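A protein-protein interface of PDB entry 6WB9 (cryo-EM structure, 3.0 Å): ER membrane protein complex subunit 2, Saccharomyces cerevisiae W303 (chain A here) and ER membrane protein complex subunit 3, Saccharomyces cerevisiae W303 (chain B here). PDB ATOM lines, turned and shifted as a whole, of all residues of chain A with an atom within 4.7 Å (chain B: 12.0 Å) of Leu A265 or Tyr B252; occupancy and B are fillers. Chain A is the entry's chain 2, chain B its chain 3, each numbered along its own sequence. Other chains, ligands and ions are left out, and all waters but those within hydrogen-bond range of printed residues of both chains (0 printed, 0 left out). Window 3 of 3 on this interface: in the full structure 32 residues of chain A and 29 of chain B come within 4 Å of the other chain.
O of Val A234 lies within hydrogen-bond range of OH of Tyr B252 (2.4 Å).
The guanidinium group of Arg B247 lies within salt-bridge range of the side-chain carboxylate of Glu A235.
The side-chain amide nitrogen of Gln B251 lies within hydrogen-bond range of the side-chain carboxylate of Glu A235, 3.2 Å away.
The backbone carbonyl oxygen (O) of Glu A238 is in hydrogen-bond range of the indole nitrogen (NE1) of Trp A244 (2.4 Å).
The side-chain carboxylate (OE2) of Glu A238 is in salt-bridge range of the side-chain amino group (NZ) of Lys A269 (2.8 Å).
OG of Ser A266 is in hydrogen-bond range of O of Trp A244 (2.6 Å).
O of Asn B243 is in hydrogen-bond range of NE of Arg B247.
Glu A235 touches Val B244.
Val B248 touches Glu A235.
Glu A235 touches Tyr B252.
CE1 of Tyr B252 touches CG of Glu A238 (3.6 Å).
Trp A244 touches Val B248 (CH2 to CG1, 3.7 Å).
Trp A244 touches Tyr B252 (CZ2 to CD2, 3.9 Å).
CD2 of Leu A262 touches OE2 of Glu B245 (3.5 Å).
CD2 of Leu A265 touches CG1 of Val B248, at 3.95 Å.
Leu A265 touches Tyr B252.
Leu A265 touches Met B253.
Of chain B, only Tyr B252 comes within 4 Å of Val A234.
No residue of chain B comes within 4 Å of Ser A237.
Of chain B, only Tyr B252 (3.6 Å) comes within 4 Å of Glu A238.
Of chain B, only Glu B245 comes within 4 Å of Leu A262.
No residue of chain B comes within 4 Å of Ser A266.
Ala A267 touches none of the printed residues of chain B.
No residue of chain B comes within 4 Å of Ser A268.
Lys A269 touches just one residue of chain B: Tyr B252 (3.7 Å).
Of the printed residues of chain A, Gln B251 touches Glu A235 (3.2 Å).
Of the printed residues of chain A, Met B253 touches Asp A261 (3.98 Å) and Leu A265 (3.8 Å).
Printed residues of chain A within 4 Å of Leu B249: Asp A261 and Leu A265.
Of the printed residues of chain A, Val B244 touches Glu A235.
The nearest residue of chain A that does not touch Tyr B252 is Ser A237 (4.2 Å).
The nearest printed residue of chain A that does not touch Gln B251 is Val A234 (5.0 Å).
Hydrophobic or aromatic side chains of chain B within 4 Å of the printed part of chain A: Val B244, Val B248, Leu B249, Tyr B252 and Met B253.
Of the 14 printed residues of chain A, 8 touch a printed residue of chain B.
Hydrophobic or aromatic side chains of chain A within 4 Å of the printed part of chain B: Trp A244, Leu A262 and Leu A265.
Among the printed residues, 17 pairs touch across the chains.
Among the printed residues, Asp or Glu carboxylates within 4 Å of a Lys or Arg side-chain nitrogen of the other chain: Glu A235 with Arg B247.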
ATOM      1  N   VAL A 234       8.989  19.825  24.404  1.00  0.00           N
ATOM      2  CA  VAL A 234       7.573  20.051  24.141  1.00  0.00           C
ATOM      3  C   VAL A 234       7.183  19.754  22.704  1.00  0.00           C
ATOM      4  O   VAL A 234       5.989  19.812  22.377  1.00  0.00           O
ATOM      5  CB  VAL A 234       7.142  21.484  24.508  1.00  0.00           C
ATOM      6  CG1 VAL A 234       7.211  21.668  25.999  1.00  0.00           C
ATOM      7  CG2 VAL A 234       8.003  22.498  23.796  1.00  0.00           C
ATOM      8  N   GLU A 235       8.140  19.442  21.836  1.00  0.00           N
ATOM      9  CA  GLU A 235       7.806  18.839  20.557  1.00  0.00           C
ATOM     10  C   GLU A 235       7.588  17.339  20.684  1.00  0.00           C
ATOM     11  O   GLU A 235       7.090  16.711  19.745  1.00  0.00           O
ATOM     12  CB  GLU A 235       8.905  19.123  19.535  1.00  0.00           C
ATOM     13  CG  GLU A 235       8.415  19.204  18.106  1.00  0.00           C
ATOM     14  CD  GLU A 235       9.513  18.933  17.107  1.00  0.00           C
ATOM     15  OE1 GLU A 235      10.677  18.784  17.530  1.00  0.00           O
ATOM     16  OE2 GLU A 235       9.213  18.867  15.897  1.00  0.00           O
ATOM     17  N   SER A 237       6.028  16.269  23.689  1.00  0.00           N
ATOM     18  CA  SER A 237       4.931  16.189  24.650  1.00  0.00           C
ATOM     19  C   SER A 237       4.241  17.540  24.707  1.00  0.00           C
ATOM     20  O   SER A 237       4.862  18.525  25.109  1.00  0.00           O
ATOM     21  CB  SER A 237       5.446  15.795  26.027  1.00  0.00           C
ATOM     22  OG  SER A 237       4.373  15.587  26.922  1.00  0.00           O
ATOM     23  N   GLU A 238       2.963  17.583  24.325  1.00  0.00           N
ATOM     24  CA  GLU A 238       2.240  18.851  24.255  1.00  0.00           C
ATOM     25  C   GLU A 238       2.016  19.449  25.638  1.00  0.00           C
ATOM     26  O   GLU A 238       2.298  20.629  25.867  1.00  0.00           O
ATOM     27  CB  GLU A 238       0.904  18.655  23.543  1.00  0.00           C
ATOM     28  CG  GLU A 238       0.000  19.873  23.586  1.00  0.00           C
ATOM     29  CD  GLU A 238      -1.442  19.546  23.266  1.00  0.00           C
ATOM     30  OE1 GLU A 238      -1.792  18.349  23.246  1.00  0.00           O
ATOM     31  OE2 GLU A 238      -2.229  20.489  23.040  1.00  0.00           O
ATOM     32  N   TRP A 244       7.339  23.384  29.030  1.00  0.00           N
ATOM     33  CA  TRP A 244       6.781  24.704  28.747  1.00  0.00           C
ATOM     34  C   TRP A 244       7.199  25.726  29.793  1.00  0.00           C
ATOM     35  O   TRP A 244       7.401  26.900  29.457  1.00  0.00           O
ATOM     36  CB  TRP A 244       5.257  24.641  28.647  1.00  0.00           C
ATOM     37  CG  TRP A 244       4.752  23.994  27.389  1.00  0.00           C
ATOM     38  CD1 TRP A 244       4.012  22.855  27.301  1.00  0.00           C
ATOM     39  CD2 TRP A 244       4.952  24.447  26.042  1.00  0.00           C
ATOM     40  NE1 TRP A 244       3.740  22.566  25.989  1.00  0.00           N
ATOM     41  CE2 TRP A 244       4.304  23.529  25.195  1.00  0.00           C
ATOM     42  CE3 TRP A 244       5.616  25.536  25.470  1.00  0.00           C
ATOM     43  CZ2 TRP A 244       4.302  23.665  23.810  1.00  0.00           C
ATOM     44  CZ3 TRP A 244       5.613  25.668  24.097  1.00  0.00           C
ATOM     45  CH2 TRP A 244       4.961  24.740  23.283  1.00  0.00           C
ATOM     46  N   ASP A 261       6.436  35.955  20.382  1.00  0.00           N
ATOM     47  CA  ASP A 261       5.914  34.810  19.634  1.00  0.00           C
ATOM     48  C   ASP A 261       6.188  33.452  20.276  1.00  0.00           C
ATOM     49  O   ASP A 261       5.663  32.450  19.788  1.00  0.00           O
ATOM     50  CB  ASP A 261       6.430  34.771  18.185  1.00  0.00           C
ATOM     51  CG  ASP A 261       5.829  35.861  17.325  1.00  0.00           C
ATOM     52  OD1 ASP A 261       4.819  36.462  17.748  1.00  0.00           O
ATOM     53  OD2 ASP A 261       6.363  36.116  16.226  1.00  0.00           O
ATOM     54  N   LEU A 262       6.959  33.380  21.361  1.00  0.00           N
ATOM     55  CA  LEU A 262       7.258  32.106  22.002  1.00  0.00           C
ATOM     56  C   LEU A 262       6.923  32.183  23.484  1.00  0.00           C
ATOM     57  O   LEU A 262       6.509  31.189  24.085  1.00  0.00           O
ATOM     58  CB  LEU A 262       8.725  31.726  21.797  1.00  0.00           C
ATOM     59  CG  LEU A 262       9.117  30.306  22.207  1.00  0.00           C
ATOM     60  CD1 LEU A 262       8.319  29.285  21.419  1.00  0.00           C
ATOM     61  CD2 LEU A 262      10.605  30.085  22.014  1.00  0.00           C
ATOM     62  N   ILE A 263       7.106  33.365  24.078  1.00  0.00           N
ATOM     63  CA  ILE A 263       6.616  33.605  25.432  1.00  0.00           C
ATOM     64  C   ILE A 263       5.093  33.600  25.442  1.00  0.00           C
ATOM     65  O   ILE A 263       4.469  33.149  26.410  1.00  0.00           O
ATOM     66  CB  ILE A 263       7.191  34.929  25.973  1.00  0.00           C
ATOM     67  CG1 ILE A 263       8.710  34.956  25.807  1.00  0.00           C
ATOM     68  CG2 ILE A 263       6.848  35.125  27.439  1.00  0.00           C
ATOM     69  CD1 ILE A 263       9.202  35.959  24.791  1.00  0.00           C
ATOM     70  N   LYS A 264       4.475  34.066  24.352  1.00  0.00           N
ATOM     71  CA  LYS A 264       3.023  34.019  24.215  1.00  0.00           C
ATOM     72  C   LYS A 264       2.527  32.580  24.104  1.00  0.00           C
ATOM     73  O   LYS A 264       1.552  32.198  24.763  1.00  0.00           O
ATOM     74  CB  LYS A 264       2.602  34.831  22.991  1.00  0.00           C
ATOM     75  CG  LYS A 264       1.103  34.970  22.794  1.00  0.00           C
ATOM     76  CD  LYS A 264       0.782  35.500  21.402  1.00  0.00           C
ATOM     77  CE  LYS A 264       1.514  36.802  21.113  1.00  0.00           C
ATOM     78  NZ  LYS A 264       1.249  37.301  19.736  1.00  0.00           N
ATOM     79  N   LEU A 265       3.204  31.766  23.288  1.00  0.00           N
ATOM     80  CA  LEU A 265       2.829  30.362  23.134  1.00  0.00           C
ATOM     81  C   LEU A 265       3.073  29.576  24.418  1.00  0.00           C
ATOM     82  O   LEU A 265       2.256  28.728  24.794  1.00  0.00           O
ATOM     83  CB  LEU A 265       3.603  29.736  21.973  1.00  0.00           C
ATOM     84  CG  LEU A 265       3.470  28.225  21.771  1.00  0.00           C
ATOM     85  CD1 LEU A 265       2.030  27.848  21.484  1.00  0.00           C
ATOM     86  CD2 LEU A 265       4.382  27.738  20.664  1.00  0.00           C
ATOM     87  N   SER A 266       4.178  29.862  25.110  1.00  0.00           N
ATOM     88  CA  SER A 266       4.468  29.170  26.360  1.00  0.00           C
ATOM     89  C   SER A 266       3.488  29.569  27.453  1.00  0.00           C
ATOM     90  O   SER A 266       3.078  28.726  28.256  1.00  0.00           O
ATOM     91  CB  SER A 266       5.900  29.455  26.800  1.00  0.00           C
ATOM     92  OG  SER A 266       6.290  28.567  27.828  1.00  0.00           O
ATOM     93  N   ALA A 267       3.076  30.839  27.478  1.00  0.00           N
ATOM     94  CA  ALA A 267       2.076  31.273  28.447  1.00  0.00           C
ATOM     95  C   ALA A 267       0.713  30.664  28.147  1.00  0.00           C
ATOM     96  O   ALA A 267      -0.014  30.280  29.070  1.00  0.00           O
ATOM     97  CB  ALA A 267       1.995  32.798  28.470  1.00  0.00           C
ATOM     98  N   SER A 268       0.367  30.532  26.861  1.00  0.00           N
ATOM     99  CA  SER A 268      -0.893  29.891  26.491  1.00  0.00           C
ATOM    100  C   SER A 268      -0.890  28.408  26.840  1.00  0.00           C
ATOM    101  O   SER A 268      -1.893  27.879  27.335  1.00  0.00           O
ATOM    102  CB  SER A 268      -1.161  30.084  25.000  1.00  0.00           C
ATOM    103  OG  SER A 268      -2.327  29.386  24.602  1.00  0.00           O
ATOM    104  N   LYS A 269       0.235  27.726  26.618  1.00  0.00           N
ATOM    105  CA  LYS A 269       0.309  26.307  26.946  1.00  0.00           C
ATOM    106  C   LYS A 269       0.354  26.073  28.450  1.00  0.00           C
ATOM    107  O   LYS A 269      -0.207  25.085  28.932  1.00  0.00           O
ATOM    108  CB  LYS A 269       1.518  25.675  26.267  1.00  0.00           C
ATOM    109  CG  LYS A 269       1.296  25.397  24.797  1.00  0.00           C
ATOM    110  CD  LYS A 269       0.196  24.375  24.601  1.00  0.00           C
ATOM    111  CE  LYS A 269      -0.049  24.108  23.131  1.00  0.00           C
ATOM    112  NZ  LYS A 269      -1.110  23.090  22.927  1.00  0.00           N
ATOM    113  N   ASN B 243      16.275  23.750  13.886  1.00  0.00           N
ATOM    114  CA  ASN B 243      15.067  24.522  13.643  1.00  0.00           C
ATOM    115  C   ASN B 243      13.893  23.959  14.432  1.00  0.00           C
ATOM    116  O   ASN B 243      12.784  23.813  13.916  1.00  0.00           O
ATOM    117  CB  ASN B 243      14.747  24.569  12.152  1.00  0.00           C
ATOM    118  CG  ASN B 243      14.759  23.200  11.514  1.00  0.00           C
ATOM    119  OD1 ASN B 243      15.659  22.398  11.759  1.00  0.00           O
ATOM    120  ND2 ASN B 243      13.750  22.918  10.699  1.00  0.00           N
ATOM    121  N   VAL B 244      14.130  23.625  15.703  1.00  0.00           N
ATOM    122  CA  VAL B 244      13.065  23.088  16.538  1.00  0.00           C
ATOM    123  C   VAL B 244      12.095  24.185  16.966  1.00  0.00           C
ATOM    124  O   VAL B 244      10.922  23.897  17.242  1.00  0.00           O
ATOM    125  CB  VAL B 244      13.677  22.329  17.739  1.00  0.00           C
ATOM    126  CG1 VAL B 244      14.292  23.280  18.759  1.00  0.00           C
ATOM    127  CG2 VAL B 244      12.659  21.398  18.389  1.00  0.00           C
ATOM    128  N   GLU B 245      12.534  25.448  16.964  1.00  0.00           N
ATOM    129  CA  GLU B 245      11.664  26.538  17.391  1.00  0.00           C
ATOM    130  C   GLU B 245      10.568  26.804  16.370  1.00  0.00           C
ATOM    131  O   GLU B 245       9.400  26.966  16.740  1.00  0.00           O
ATOM    132  CB  GLU B 245      12.485  27.802  17.635  1.00  0.00           C
ATOM    133  CG  GLU B 245      11.682  28.949  18.218  1.00  0.00           C
ATOM    134  CD  GLU B 245      12.545  30.137  18.585  1.00  0.00           C
ATOM    135  OE1 GLU B 245      13.782  30.043  18.440  1.00  0.00           O
ATOM    136  OE2 GLU B 245      11.987  31.165  19.019  1.00  0.00           O
ATOM    137  N   GLN B 246      10.915  26.814  15.080  1.00  0.00           N
ATOM    138  CA  GLN B 246       9.896  27.009  14.056  1.00  0.00           C
ATOM    139  C   GLN B 246       8.988  25.791  13.931  1.00  0.00           C
ATOM    140  O   GLN B 246       7.819  25.935  13.566  1.00  0.00           O
ATOM    141  CB  GLN B 246      10.542  27.348  12.710  1.00  0.00           C
ATOM    142  CG  GLN B 246      11.427  26.264  12.126  1.00  0.00           C
ATOM    143  CD  GLN B 246      11.993  26.644  10.772  1.00  0.00           C
ATOM    144  OE1 GLN B 246      12.122  27.824  10.450  1.00  0.00           O
ATOM    145  NE2 GLN B 246      12.329  25.642   9.969  1.00  0.00           N
ATOM    146  N   ARG B 247       9.481  24.602  14.287  1.00  0.00           N
ATOM    147  CA  ARG B 247       8.621  23.422  14.285  1.00  0.00           C
ATOM    148  C   ARG B 247       7.617  23.465  15.431  1.00  0.00           C
ATOM    149  O   ARG B 247       6.452  23.087  15.254  1.00  0.00           O
ATOM    150  CB  ARG B 247       9.467  22.152  14.351  1.00  0.00           C
ATOM    151  CG  ARG B 247       9.988  21.707  13.000  1.00  0.00           C
ATOM    152  CD  ARG B 247      10.707  20.371  13.071  1.00  0.00           C
ATOM    153  NE  ARG B 247      12.143  20.530  13.279  1.00  0.00           N
ATOM    154  CZ  ARG B 247      12.778  20.210  14.401  1.00  0.00           C
ATOM    155  NH1 ARG B 247      12.108  19.703  15.422  1.00  0.00           N
ATOM    156  NH2 ARG B 247      14.086  20.392  14.497  1.00  0.00           N
ATOM    157  N   VAL B 248       8.044  23.933  16.609  1.00  0.00           N
ATOM    158  CA  VAL B 248       7.109  24.113  17.717  1.00  0.00           C
ATOM    159  C   VAL B 248       6.112  25.228  17.402  1.00  0.00           C
ATOM    160  O   VAL B 248       4.921  25.117  17.729  1.00  0.00           O
ATOM    161  CB  VAL B 248       7.892  24.363  19.023  1.00  0.00           C
ATOM    162  CG1 VAL B 248       6.983  24.808  20.160  1.00  0.00           C
ATOM    163  CG2 VAL B 248       8.614  23.101  19.433  1.00  0.00           C
ATOM    164  N   LEU B 249       6.554  26.280  16.708  1.00  0.00           N
ATOM    165  CA  LEU B 249       5.635  27.346  16.315  1.00  0.00           C
ATOM    166  C   LEU B 249       4.660  26.896  15.232  1.00  0.00           C
ATOM    167  O   LEU B 249       3.539  27.409  15.161  1.00  0.00           O
ATOM    168  CB  LEU B 249       6.420  28.569  15.843  1.00  0.00           C
ATOM    169  CG  LEU B 249       7.150  29.344  16.938  1.00  0.00           C
ATOM    170  CD1 LEU B 249       7.839  30.569  16.367  1.00  0.00           C
ATOM    171  CD2 LEU B 249       6.185  29.727  18.032  1.00  0.00           C
ATOM    172  N   LYS B 250       5.061  25.949  14.382  1.00  0.00           N
ATOM    173  CA  LYS B 250       4.131  25.412  13.395  1.00  0.00           C
ATOM    174  C   LYS B 250       3.138  24.450  14.032  1.00  0.00           C
ATOM    175  O   LYS B 250       1.973  24.395  13.623  1.00  0.00           O
ATOM    176  CB  LYS B 250       4.888  24.713  12.268  1.00  0.00           C
ATOM    177  CG  LYS B 250       5.499  25.646  11.239  1.00  0.00           C
ATOM    178  CD  LYS B 250       6.049  24.868  10.055  1.00  0.00           C
ATOM    179  CE  LYS B 250       7.087  23.846  10.491  1.00  0.00           C
ATOM    180  NZ  LYS B 250       7.535  22.997   9.355  1.00  0.00           N
ATOM    181  N   GLN B 251       3.579  23.677  15.028  1.00  0.00           N
ATOM    182  CA  GLN B 251       2.712  22.647  15.595  1.00  0.00           C
ATOM    183  C   GLN B 251       1.635  23.245  16.492  1.00  0.00           C
ATOM    184  O   GLN B 251       0.445  22.958  16.323  1.00  0.00           O
ATOM    185  CB  GLN B 251       3.543  21.625  16.369  1.00  0.00           C
ATOM    186  CG  GLN B 251       4.267  20.625  15.492  1.00  0.00           C
ATOM    187  CD  GLN B 251       5.083  19.639  16.297  1.00  0.00           C
ATOM    188  OE1 GLN B 251       4.869  19.473  17.496  1.00  0.00           O
ATOM    189  NE2 GLN B 251       6.030  18.980  15.641  1.00  0.00           N
ATOM    190  N   TYR B 252       2.029  24.080  17.451  1.00  0.00           N
ATOM    191  CA  TYR B 252       1.113  24.556  18.478  1.00  0.00           C
ATOM    192  C   TYR B 252       0.599  25.963  18.215  1.00  0.00           C
ATOM    193  O   TYR B 252      -0.002  26.567  19.108  1.00  0.00           O
ATOM    194  CB  TYR B 252       1.789  24.493  19.847  1.00  0.00           C
ATOM    195  CG  TYR B 252       2.392  23.146  20.152  1.00  0.00           C
ATOM    196  CD1 TYR B 252       1.596  22.083  20.554  1.00  0.00           C
ATOM    197  CD2 TYR B 252       3.758  22.934  20.032  1.00  0.00           C
ATOM    198  CE1 TYR B 252       2.143  20.849  20.828  1.00  0.00           C
ATOM    199  CE2 TYR B 252       4.312  21.703  20.305  1.00  0.00           C
ATOM    200  CZ  TYR B 252       3.500  20.667  20.701  1.00  0.00           C
ATOM    201  OH  TYR B 252       4.051  19.440  20.975  1.00  0.00           O
ATOM    202  N   MET B 253       0.810  26.496  17.018  1.00  0.00           N
ATOM    203  CA  MET B 253       0.311  27.821  16.674  1.00  0.00           C
ATOM    204  C   MET B 253       0.018  27.931  15.181  1.00  0.00           C
ATOM    205  O   MET B 253      -0.655  27.075  14.605  1.00  0.00           O
ATOM    206  CB  MET B 253       1.316  28.894  17.091  1.00  0.00           C
ATOM    207  CG  MET B 253       0.865  29.751  18.257  1.00  0.00           C
ATOM    208  SD  MET B 253       2.128  30.944  18.732  1.00  0.00           S
ATOM    209  CE  MET B 253       2.573  31.609  17.132  1.00  0.00           C
